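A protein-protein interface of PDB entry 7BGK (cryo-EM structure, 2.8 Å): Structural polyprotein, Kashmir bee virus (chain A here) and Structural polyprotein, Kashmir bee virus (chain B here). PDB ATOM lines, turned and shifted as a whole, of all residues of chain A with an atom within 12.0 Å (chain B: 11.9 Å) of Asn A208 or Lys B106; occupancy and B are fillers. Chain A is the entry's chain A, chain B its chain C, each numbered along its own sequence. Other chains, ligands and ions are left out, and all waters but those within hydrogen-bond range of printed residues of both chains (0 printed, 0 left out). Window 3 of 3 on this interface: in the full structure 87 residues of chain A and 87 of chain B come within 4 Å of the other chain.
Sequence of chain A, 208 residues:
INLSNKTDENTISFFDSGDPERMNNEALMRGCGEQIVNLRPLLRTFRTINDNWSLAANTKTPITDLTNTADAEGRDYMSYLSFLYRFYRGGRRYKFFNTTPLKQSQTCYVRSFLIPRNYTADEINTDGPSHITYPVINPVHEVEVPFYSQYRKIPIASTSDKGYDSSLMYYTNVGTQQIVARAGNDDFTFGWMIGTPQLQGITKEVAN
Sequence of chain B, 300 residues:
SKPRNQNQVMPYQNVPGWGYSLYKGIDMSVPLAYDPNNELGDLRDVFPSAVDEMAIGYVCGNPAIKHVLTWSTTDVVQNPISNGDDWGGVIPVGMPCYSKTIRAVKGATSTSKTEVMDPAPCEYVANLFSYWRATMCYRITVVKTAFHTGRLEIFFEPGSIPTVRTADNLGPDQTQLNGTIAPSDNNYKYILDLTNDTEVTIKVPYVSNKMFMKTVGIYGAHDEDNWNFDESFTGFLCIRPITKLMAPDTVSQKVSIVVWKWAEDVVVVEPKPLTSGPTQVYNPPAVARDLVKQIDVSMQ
Of the 6 printed residues of chain A, 5 touch a printed residue of chain B.
Hydrophobic or aromatic side chains of chain A that line the printed part of chain B: Val A206.
Among the printed residues, 13 pairs touch across the chains.
Among the printed residues, no Asp or Glu carboxylate lies within 4 Å of a Lys or Arg side-chain nitrogen of the other chain.
Of the printed residues of chain B, Thr A203 touches Ser B112 (3.4 Å), Lys B113 (3.7 Å) and Thr B114 (3.6 Å).
Of the printed residues of chain B, Lys A204 touches Thr B111 (3.8 Å), Ser B112 (2.5 Å) and Lys B113 (3.3 Å).
Ala A207 touches none of the printed residues of chain B.
Of chain B, only Lys B106 and Ser B110 come within 4 Å of Asn A208.
No residue of chain A comes within 4 Å of Ala B104.
No residue of chain A comes within 4 Å of Val B105.
Lys B106 touches just one residue of chain A: Asn A208 (3.5 Å).
No residue of chain A comes within 4 Å of Gly B107.
Of chain A, only Glu A205, Val A206 and Asn A208 come within 4 Å of Ser B110.
Of chain A, only Lys A204 (3.8 Å), Glu A205 (3.2 Å) and Val A206 (2.8 Å) come within 4 Å of Thr B111.
Printed residues of chain A within 4 Å of Lys B113: Thr A203 and Lys A204.
Leu B291 touches none of the printed residues of chain A.
The nearest residue of chain B that does not touch Asn A208 is Thr B111 (4.4 Å).
The nearest residue of chain A that does not touch Lys B106 is Ala A207 (7.5 Å).
The nearest printed residue of chain A that does not touch Thr B114 is Lys A204 (5.1 Å).
The side-chain amino group (NZ) of Lys B113 is in salt-bridge range of the side-chain carboxylate (OD2) of Asp B168, at 3.6 Å.
The backbone NH (N) of Arg B103 lies within hydrogen-bond range of the backbone carbonyl oxygen (O) of Thr B114, 2.4 Å away.
O of Val B105 is in hydrogen-bond range of N of Ser B112 (3.4 Å).
Among the printed residues, pairs that only touch across the chains: Thr A203 with Ser B112, Thr A203 with Lys B113, Thr A203 with Thr B114, Lys A204 with Thr B111, Glu A205 with Thr B111, Val A206 with Ser B110 and Asn A208 with Ser B110.
The backbone NH (N) of Val A206 is in hydrogen-bond range of the backbone carbonyl oxygen (O) of Thr B111, 2.8 Å away.
O of Ser B112 sits close to N of Lys A204.
OE2 of Glu A205 sits at hydrogen-bond distance from OG of Ser B110.
The backbone NH (N) of Lys A204 lies within hydrogen-bond range of the backbone carbonyl oxygen (O) of Lys B113, 3.3 Å away.
N of Glu A205 lies within hydrogen-bond range of O of Ser B112, 3.3 Å away.
The side-chain amino group of Lys B106 lies close to the side-chain amide nitrogen of Asn A208, at 3.5 Å.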
ATOM      1  N   THR A 203      27.388  11.453 -15.205  1.00  0.00           N
ATOM      2  CA  THR A 203      27.694  10.793 -16.466  1.00  0.00           C
ATOM      3  C   THR A 203      28.878   9.861 -16.252  1.00  0.00           C
ATOM      4  O   THR A 203      29.933  10.293 -15.776  1.00  0.00           O
ATOM      5  CB  THR A 203      28.001  11.805 -17.569  1.00  0.00           C
ATOM      6  OG1 THR A 203      26.944  12.769 -17.642  1.00  0.00           O
ATOM      7  CG2 THR A 203      28.108  11.114 -18.904  1.00  0.00           C
ATOM      8  N   LYS A 204      28.704   8.591 -16.605  1.00  0.00           N
ATOM      9  CA  LYS A 204      29.705   7.546 -16.394  1.00  0.00           C
ATOM     10  C   LYS A 204      30.046   6.952 -17.754  1.00  0.00           C
ATOM     11  O   LYS A 204      29.339   6.068 -18.245  1.00  0.00           O
ATOM     12  CB  LYS A 204      29.191   6.464 -15.448  1.00  0.00           C
ATOM     13  CG  LYS A 204      28.538   6.974 -14.184  1.00  0.00           C
ATOM     14  CD  LYS A 204      27.876   5.843 -13.412  1.00  0.00           C
ATOM     15  CE  LYS A 204      27.415   6.298 -12.035  1.00  0.00           C
ATOM     16  NZ  LYS A 204      26.021   5.871 -11.717  1.00  0.00           N
ATOM     17  N   GLU A 205      31.133   7.420 -18.360  1.00  0.00           N
ATOM     18  CA  GLU A 205      31.615   6.821 -19.599  1.00  0.00           C
ATOM     19  C   GLU A 205      32.288   5.496 -19.274  1.00  0.00           C
ATOM     20  O   GLU A 205      33.357   5.467 -18.659  1.00  0.00           O
ATOM     21  CB  GLU A 205      32.580   7.762 -20.313  1.00  0.00           C
ATOM     22  CG  GLU A 205      32.851   7.376 -21.753  1.00  0.00           C
ATOM     23  CD  GLU A 205      33.756   8.364 -22.458  1.00  0.00           C
ATOM     24  OE1 GLU A 205      34.056   9.422 -21.867  1.00  0.00           O
ATOM     25  OE2 GLU A 205      34.167   8.080 -23.602  1.00  0.00           O
ATOM     26  N   VAL A 206      31.660   4.400 -19.687  1.00  0.00           N
ATOM     27  CA  VAL A 206      32.118   3.053 -19.378  1.00  0.00           C
ATOM     28  C   VAL A 206      32.669   2.430 -20.652  1.00  0.00           C
ATOM     29  O   VAL A 206      32.142   2.662 -21.746  1.00  0.00           O
ATOM     30  CB  VAL A 206      30.988   2.189 -18.784  1.00  0.00           C
ATOM     31  CG1 VAL A 206      29.836   2.067 -19.762  1.00  0.00           C
ATOM     32  CG2 VAL A 206      31.515   0.811 -18.393  1.00  0.00           C
ATOM     33  N   ALA A 207      33.723   1.633 -20.508  1.00  0.00           N
ATOM     34  CA  ALA A 207      34.265   0.890 -21.634  1.00  0.00           C
ATOM     35  C   ALA A 207      33.384  -0.317 -21.927  1.00  0.00           C
ATOM     36  O   ALA A 207      33.066  -1.101 -21.027  1.00  0.00           O
ATOM     37  CB  ALA A 207      35.696   0.446 -21.338  1.00  0.00           C
ATOM     38  N   ASN A 208      32.990  -0.461 -23.188  1.00  0.00           N
ATOM     39  CA  ASN A 208      32.034  -1.488 -23.581  1.00  0.00           C
ATOM     40  C   ASN A 208      32.736  -2.791 -23.955  1.00  0.00           C
ATOM     41  O   ASN A 208      33.908  -2.793 -24.331  1.00  0.00           O
ATOM     42  CB  ASN A 208      31.175  -0.993 -24.745  1.00  0.00           C
ATOM     43  CG  ASN A 208      31.993  -0.663 -25.978  1.00  0.00           C
ATOM     44  OD1 ASN A 208      33.194  -0.918 -26.032  1.00  0.00           O
ATOM     45  ND2 ASN A 208      31.339  -0.087 -26.980  1.00  0.00           N
ATOM     46  N   ILE B 102      18.609   6.029 -17.333  1.00  0.00           N
ATOM     47  CA  ILE B 102      19.939   6.183 -17.901  1.00  0.00           C
ATOM     48  C   ILE B 102      19.808   6.314 -19.409  1.00  0.00           C
ATOM     49  O   ILE B 102      19.254   5.432 -20.074  1.00  0.00           O
ATOM     50  CB  ILE B 102      20.849   5.004 -17.532  1.00  0.00           C
ATOM     51  CG1 ILE B 102      20.670   4.612 -16.063  1.00  0.00           C
ATOM     52  CG2 ILE B 102      22.283   5.359 -17.806  1.00  0.00           C
ATOM     53  CD1 ILE B 102      20.937   5.723 -15.080  1.00  0.00           C
ATOM     54  N   ARG B 103      20.303   7.424 -19.944  1.00  0.00           N
ATOM     55  CA  ARG B 103      20.418   7.618 -21.381  1.00  0.00           C
ATOM     56  C   ARG B 103      21.803   7.170 -21.825  1.00  0.00           C
ATOM     57  O   ARG B 103      22.811   7.760 -21.422  1.00  0.00           O
ATOM     58  CB  ARG B 103      20.181   9.077 -21.749  1.00  0.00           C
ATOM     59  CG  ARG B 103      20.366   9.385 -23.210  1.00  0.00           C
ATOM     60  CD  ARG B 103      20.072  10.824 -23.487  1.00  0.00           C
ATOM     61  NE  ARG B 103      20.159  11.152 -24.905  1.00  0.00           N
ATOM     62  CZ  ARG B 103      21.294  11.405 -25.542  1.00  0.00           C
ATOM     63  NH1 ARG B 103      21.273  11.703 -26.827  1.00  0.00           N
ATOM     64  NH2 ARG B 103      22.448  11.363 -24.900  1.00  0.00           N
ATOM     65  N   ALA B 104      21.850   6.135 -22.654  1.00  0.00           N
ATOM     66  CA  ALA B 104      23.095   5.573 -23.150  1.00  0.00           C
ATOM     67  C   ALA B 104      23.282   5.961 -24.608  1.00  0.00           C
ATOM     68  O   ALA B 104      22.329   5.940 -25.391  1.00  0.00           O
ATOM     69  CB  ALA B 104      23.102   4.052 -23.011  1.00  0.00           C
ATOM     70  N   VAL B 105      24.510   6.326 -24.966  1.00  0.00           N
ATOM     71  CA  VAL B 105      24.866   6.618 -26.348  1.00  0.00           C
ATOM     72  C   VAL B 105      26.182   5.924 -26.641  1.00  0.00           C
ATOM     73  O   VAL B 105      27.159   6.108 -25.907  1.00  0.00           O
ATOM     74  CB  VAL B 105      24.996   8.130 -26.602  1.00  0.00           C
ATOM     75  CG1 VAL B 105      25.313   8.402 -28.060  1.00  0.00           C
ATOM     76  CG2 VAL B 105      23.762   8.856 -26.145  1.00  0.00           C
ATOM     77  N   LYS B 106      26.216   5.144 -27.712  1.00  0.00           N
ATOM     78  CA  LYS B 106      27.391   4.365 -28.059  1.00  0.00           C
ATOM     79  C   LYS B 106      28.146   4.981 -29.225  1.00  0.00           C
ATOM     80  O   LYS B 106      27.571   5.665 -30.075  1.00  0.00           O
ATOM     81  CB  LYS B 106      27.013   2.931 -28.395  1.00  0.00           C
ATOM     82  CG  LYS B 106      26.526   2.168 -27.189  1.00  0.00           C
ATOM     83  CD  LYS B 106      26.187   0.721 -27.485  1.00  0.00           C
ATOM     84  CE  LYS B 106      27.389  -0.056 -28.014  1.00  0.00           C
ATOM     85  NZ  LYS B 106      27.991  -1.002 -27.032  1.00  0.00           N
ATOM     86  N   GLY B 107      29.449   4.721 -29.257  1.00  0.00           N
ATOM     87  CA  GLY B 107      30.313   5.252 -30.293  1.00  0.00           C
ATOM     88  C   GLY B 107      31.772   4.895 -30.081  1.00  0.00           C
ATOM     89  O   GLY B 107      32.168   3.738 -30.238  1.00  0.00           O
ATOM     90  N   SER B 110      32.636   3.231 -27.032  1.00  0.00           N
ATOM     91  CA  SER B 110      32.225   3.190 -25.635  1.00  0.00           C
ATOM     92  C   SER B 110      30.889   3.885 -25.434  1.00  0.00           C
ATOM     93  O   SER B 110      30.332   4.469 -26.365  1.00  0.00           O
ATOM     94  CB  SER B 110      33.279   3.845 -24.745  1.00  0.00           C
ATOM     95  OG  SER B 110      33.384   5.229 -25.020  1.00  0.00           O
ATOM     96  N   THR B 111      30.380   3.817 -24.207  1.00  0.00           N
ATOM     97  CA  THR B 111      29.075   4.357 -23.859  1.00  0.00           C
ATOM     98  C   THR B 111      29.237   5.367 -22.732  1.00  0.00           C
ATOM     99  O   THR B 111      30.099   5.215 -21.866  1.00  0.00           O
ATOM    100  CB  THR B 111      28.115   3.244 -23.434  1.00  0.00           C
ATOM    101  OG1 THR B 111      28.135   2.193 -24.403  1.00  0.00           O
ATOM    102  CG2 THR B 111      26.704   3.769 -23.314  1.00  0.00           C
ATOM    103  N   SER B 112      28.399   6.402 -22.749  1.00  0.00           N
ATOM    104  CA  SER B 112      28.523   7.519 -21.819  1.00  0.00           C
ATOM    105  C   SER B 112      27.617   7.395 -20.602  1.00  0.00           C
ATOM    106  O   SER B 112      28.010   7.802 -19.506  1.00  0.00           O
ATOM    107  CB  SER B 112      28.245   8.836 -22.538  1.00  0.00           C
ATOM    108  OG  SER B 112      29.102   8.979 -23.656  1.00  0.00           O
ATOM    109  N   LYS B 113      26.404   6.865 -20.761  1.00  0.00           N
ATOM    110  CA  LYS B 113      25.534   6.537 -19.631  1.00  0.00           C
ATOM    111  C   LYS B 113      25.220   7.779 -18.789  1.00  0.00           C
ATOM    112  O   LYS B 113      25.640   7.920 -17.641  1.00  0.00           O
ATOM    113  CB  LYS B 113      26.163   5.441 -18.767  1.00  0.00           C
ATOM    114  CG  LYS B 113      26.254   4.086 -19.430  1.00  0.00           C
ATOM    115  CD  LYS B 113      24.988   3.289 -19.229  1.00  0.00           C
ATOM    116  CE  LYS B 113      25.148   1.863 -19.707  1.00  0.00           C
ATOM    117  NZ  LYS B 113      23.889   1.088 -19.572  1.00  0.00           N
ATOM    118  N   THR B 114      24.469   8.684 -19.406  1.00  0.00           N
ATOM    119  CA  THR B 114      23.940   9.855 -18.721  1.00  0.00           C
ATOM    120  C   THR B 114      22.624   9.515 -18.035  1.00  0.00           C
ATOM    121  O   THR B 114      21.769   8.836 -18.609  1.00  0.00           O
ATOM    122  CB  THR B 114      23.725  10.999 -19.709  1.00  0.00           C
ATOM    123  OG1 THR B 114      24.913  11.198 -20.482  1.00  0.00           O
ATOM    124  CG2 THR B 114      23.381  12.270 -18.983  1.00  0.00           C
ATOM    125  N   ASP B 168      23.980   1.166 -12.483  1.00  0.00           N
ATOM    126  CA  ASP B 168      23.742   2.558 -12.828  1.00  0.00           C
ATOM    127  C   ASP B 168      22.481   3.148 -12.220  1.00  0.00           C
ATOM    128  O   ASP B 168      22.326   4.372 -12.258  1.00  0.00           O
ATOM    129  CB  ASP B 168      23.668   2.722 -14.353  1.00  0.00           C
ATOM    130  CG  ASP B 168      22.726   1.731 -15.001  1.00  0.00           C
ATOM    131  OD1 ASP B 168      22.013   1.019 -14.265  1.00  0.00           O
ATOM    132  OD2 ASP B 168      22.700   1.664 -16.247  1.00  0.00           O
ATOM    133  N   PRO B 285      18.704  16.445 -26.399  1.00  0.00           N
ATOM    134  CA  PRO B 285      19.282  16.663 -27.724  1.00  0.00           C
ATOM    135  C   PRO B 285      18.326  16.232 -28.822  1.00  0.00           C
ATOM    136  O   PRO B 285      17.347  15.520 -28.596  1.00  0.00           O
ATOM    137  CB  PRO B 285      20.543  15.800 -27.705  1.00  0.00           C
ATOM    138  CG  PRO B 285      20.269  14.759 -26.712  1.00  0.00           C
ATOM    139  CD  PRO B 285      19.404  15.373 -25.673  1.00  0.00           C
ATOM    140  N   VAL B 287      18.765  14.285 -31.764  1.00  0.00           N
ATOM    141  CA  VAL B 287      18.784  12.879 -32.117  1.00  0.00           C
ATOM    142  C   VAL B 287      19.357  12.086 -30.955  1.00  0.00           C
ATOM    143  O   VAL B 287      20.058  12.613 -30.086  1.00  0.00           O
ATOM    144  CB  VAL B 287      19.596  12.625 -33.412  1.00  0.00           C
ATOM    145  CG1 VAL B 287      19.349  11.218 -33.948  1.00  0.00           C
ATOM    146  CG2 VAL B 287      19.260  13.655 -34.470  1.00  0.00           C
ATOM    147  N   ALA B 288      19.043  10.792 -30.935  1.00  0.00           N
ATOM    148  CA  ALA B 288      19.534   9.919 -29.881  1.00  0.00           C
ATOM    149  C   ALA B 288      21.026   9.653 -30.018  1.00  0.00           C
ATOM    150  O   ALA B 288      21.659   9.238 -29.042  1.00  0.00           O
ATOM    151  CB  ALA B 288      18.758   8.605 -29.889  1.00  0.00           C
ATOM    152  N   ARG B 289      21.599   9.872 -31.205  1.00  0.00           N
ATOM    153  CA  ARG B 289      23.039   9.727 -31.368  1.00  0.00           C
ATOM    154  C   ARG B 289      23.808  10.877 -30.739  1.00  0.00           C
ATOM    155  O   ARG B 289      25.021  10.760 -30.540  1.00  0.00           O
ATOM    156  CB  ARG B 289      23.420   9.683 -32.852  1.00  0.00           C
ATOM    157  CG  ARG B 289      23.157  11.005 -33.593  1.00  0.00           C
ATOM    158  CD  ARG B 289      23.842  11.063 -34.952  1.00  0.00           C
ATOM    159  NE  ARG B 289      23.916  12.438 -35.451  1.00  0.00           N
ATOM    160  CZ  ARG B 289      23.207  12.935 -36.462  1.00  0.00           C
ATOM    161  NH1 ARG B 289      22.336  12.186 -37.126  1.00  0.00           N
ATOM    162  NH2 ARG B 289      23.373  14.204 -36.811  1.00  0.00           N
ATOM    163  N   ASP B 290      23.135  11.976 -30.425  1.00  0.00           N
ATOM    164  CA  ASP B 290      23.811  13.168 -29.943  1.00  0.00           C
ATOM    165  C   ASP B 290      24.205  13.033 -28.481  1.00  0.00           C
ATOM    166  O   ASP B 290      23.455  12.493 -27.664  1.00  0.00           O
ATOM    167  CB  ASP B 290      22.916  14.392 -30.124  1.00  0.00           C
ATOM    168  CG  ASP B 290      22.757  14.789 -31.576  1.00  0.00           C
ATOM    169  OD1 ASP B 290      23.684  14.533 -32.372  1.00  0.00           O
ATOM    170  OD2 ASP B 290      21.707  15.371 -31.920  1.00  0.00           O
ATOM    171  N   LEU B 291      25.392  13.528 -28.160  1.00  0.00           N
ATOM    172  CA  LEU B 291      25.868  13.551 -26.789  1.00  0.00           C
ATOM    173  C   LEU B 291      25.344  14.795 -26.084  1.00  0.00           C
ATOM    174  O   LEU B 291      25.095  15.832 -26.703  1.00  0.00           O
ATOM    175  CB  LEU B 291      27.394  13.511 -26.736  1.00  0.00           C
ATOM    176  CG  LEU B 291      28.018  12.112 -26.678  1.00  0.00           C
ATOM    177  CD1 LEU B 291      27.901  11.394 -28.004  1.00  0.00           C
ATOM    178  CD2 LEU B 291      29.470  12.194 -26.241  1.00  0.00           C
ATOM    179  N   VAL B 292      25.177  14.676 -24.772  1.00  0.00           N
ATOM    180  CA  VAL B 292      24.595  15.752 -23.986  1.00  0.00           C
ATOM    181  C   VAL B 292      25.668  16.765 -23.599  1.00  0.00           C
ATOM    182  O   VAL B 292      26.871  16.498 -23.648  1.00  0.00           O
ATOM    183  CB  VAL B 292      23.874  15.202 -22.745  1.00  0.00           C
ATOM    184  CG1 VAL B 292      22.840  14.183 -23.150  1.00  0.00           C
ATOM    185  CG2 VAL B 292      24.861  14.591 -21.778  1.00  0.00           C
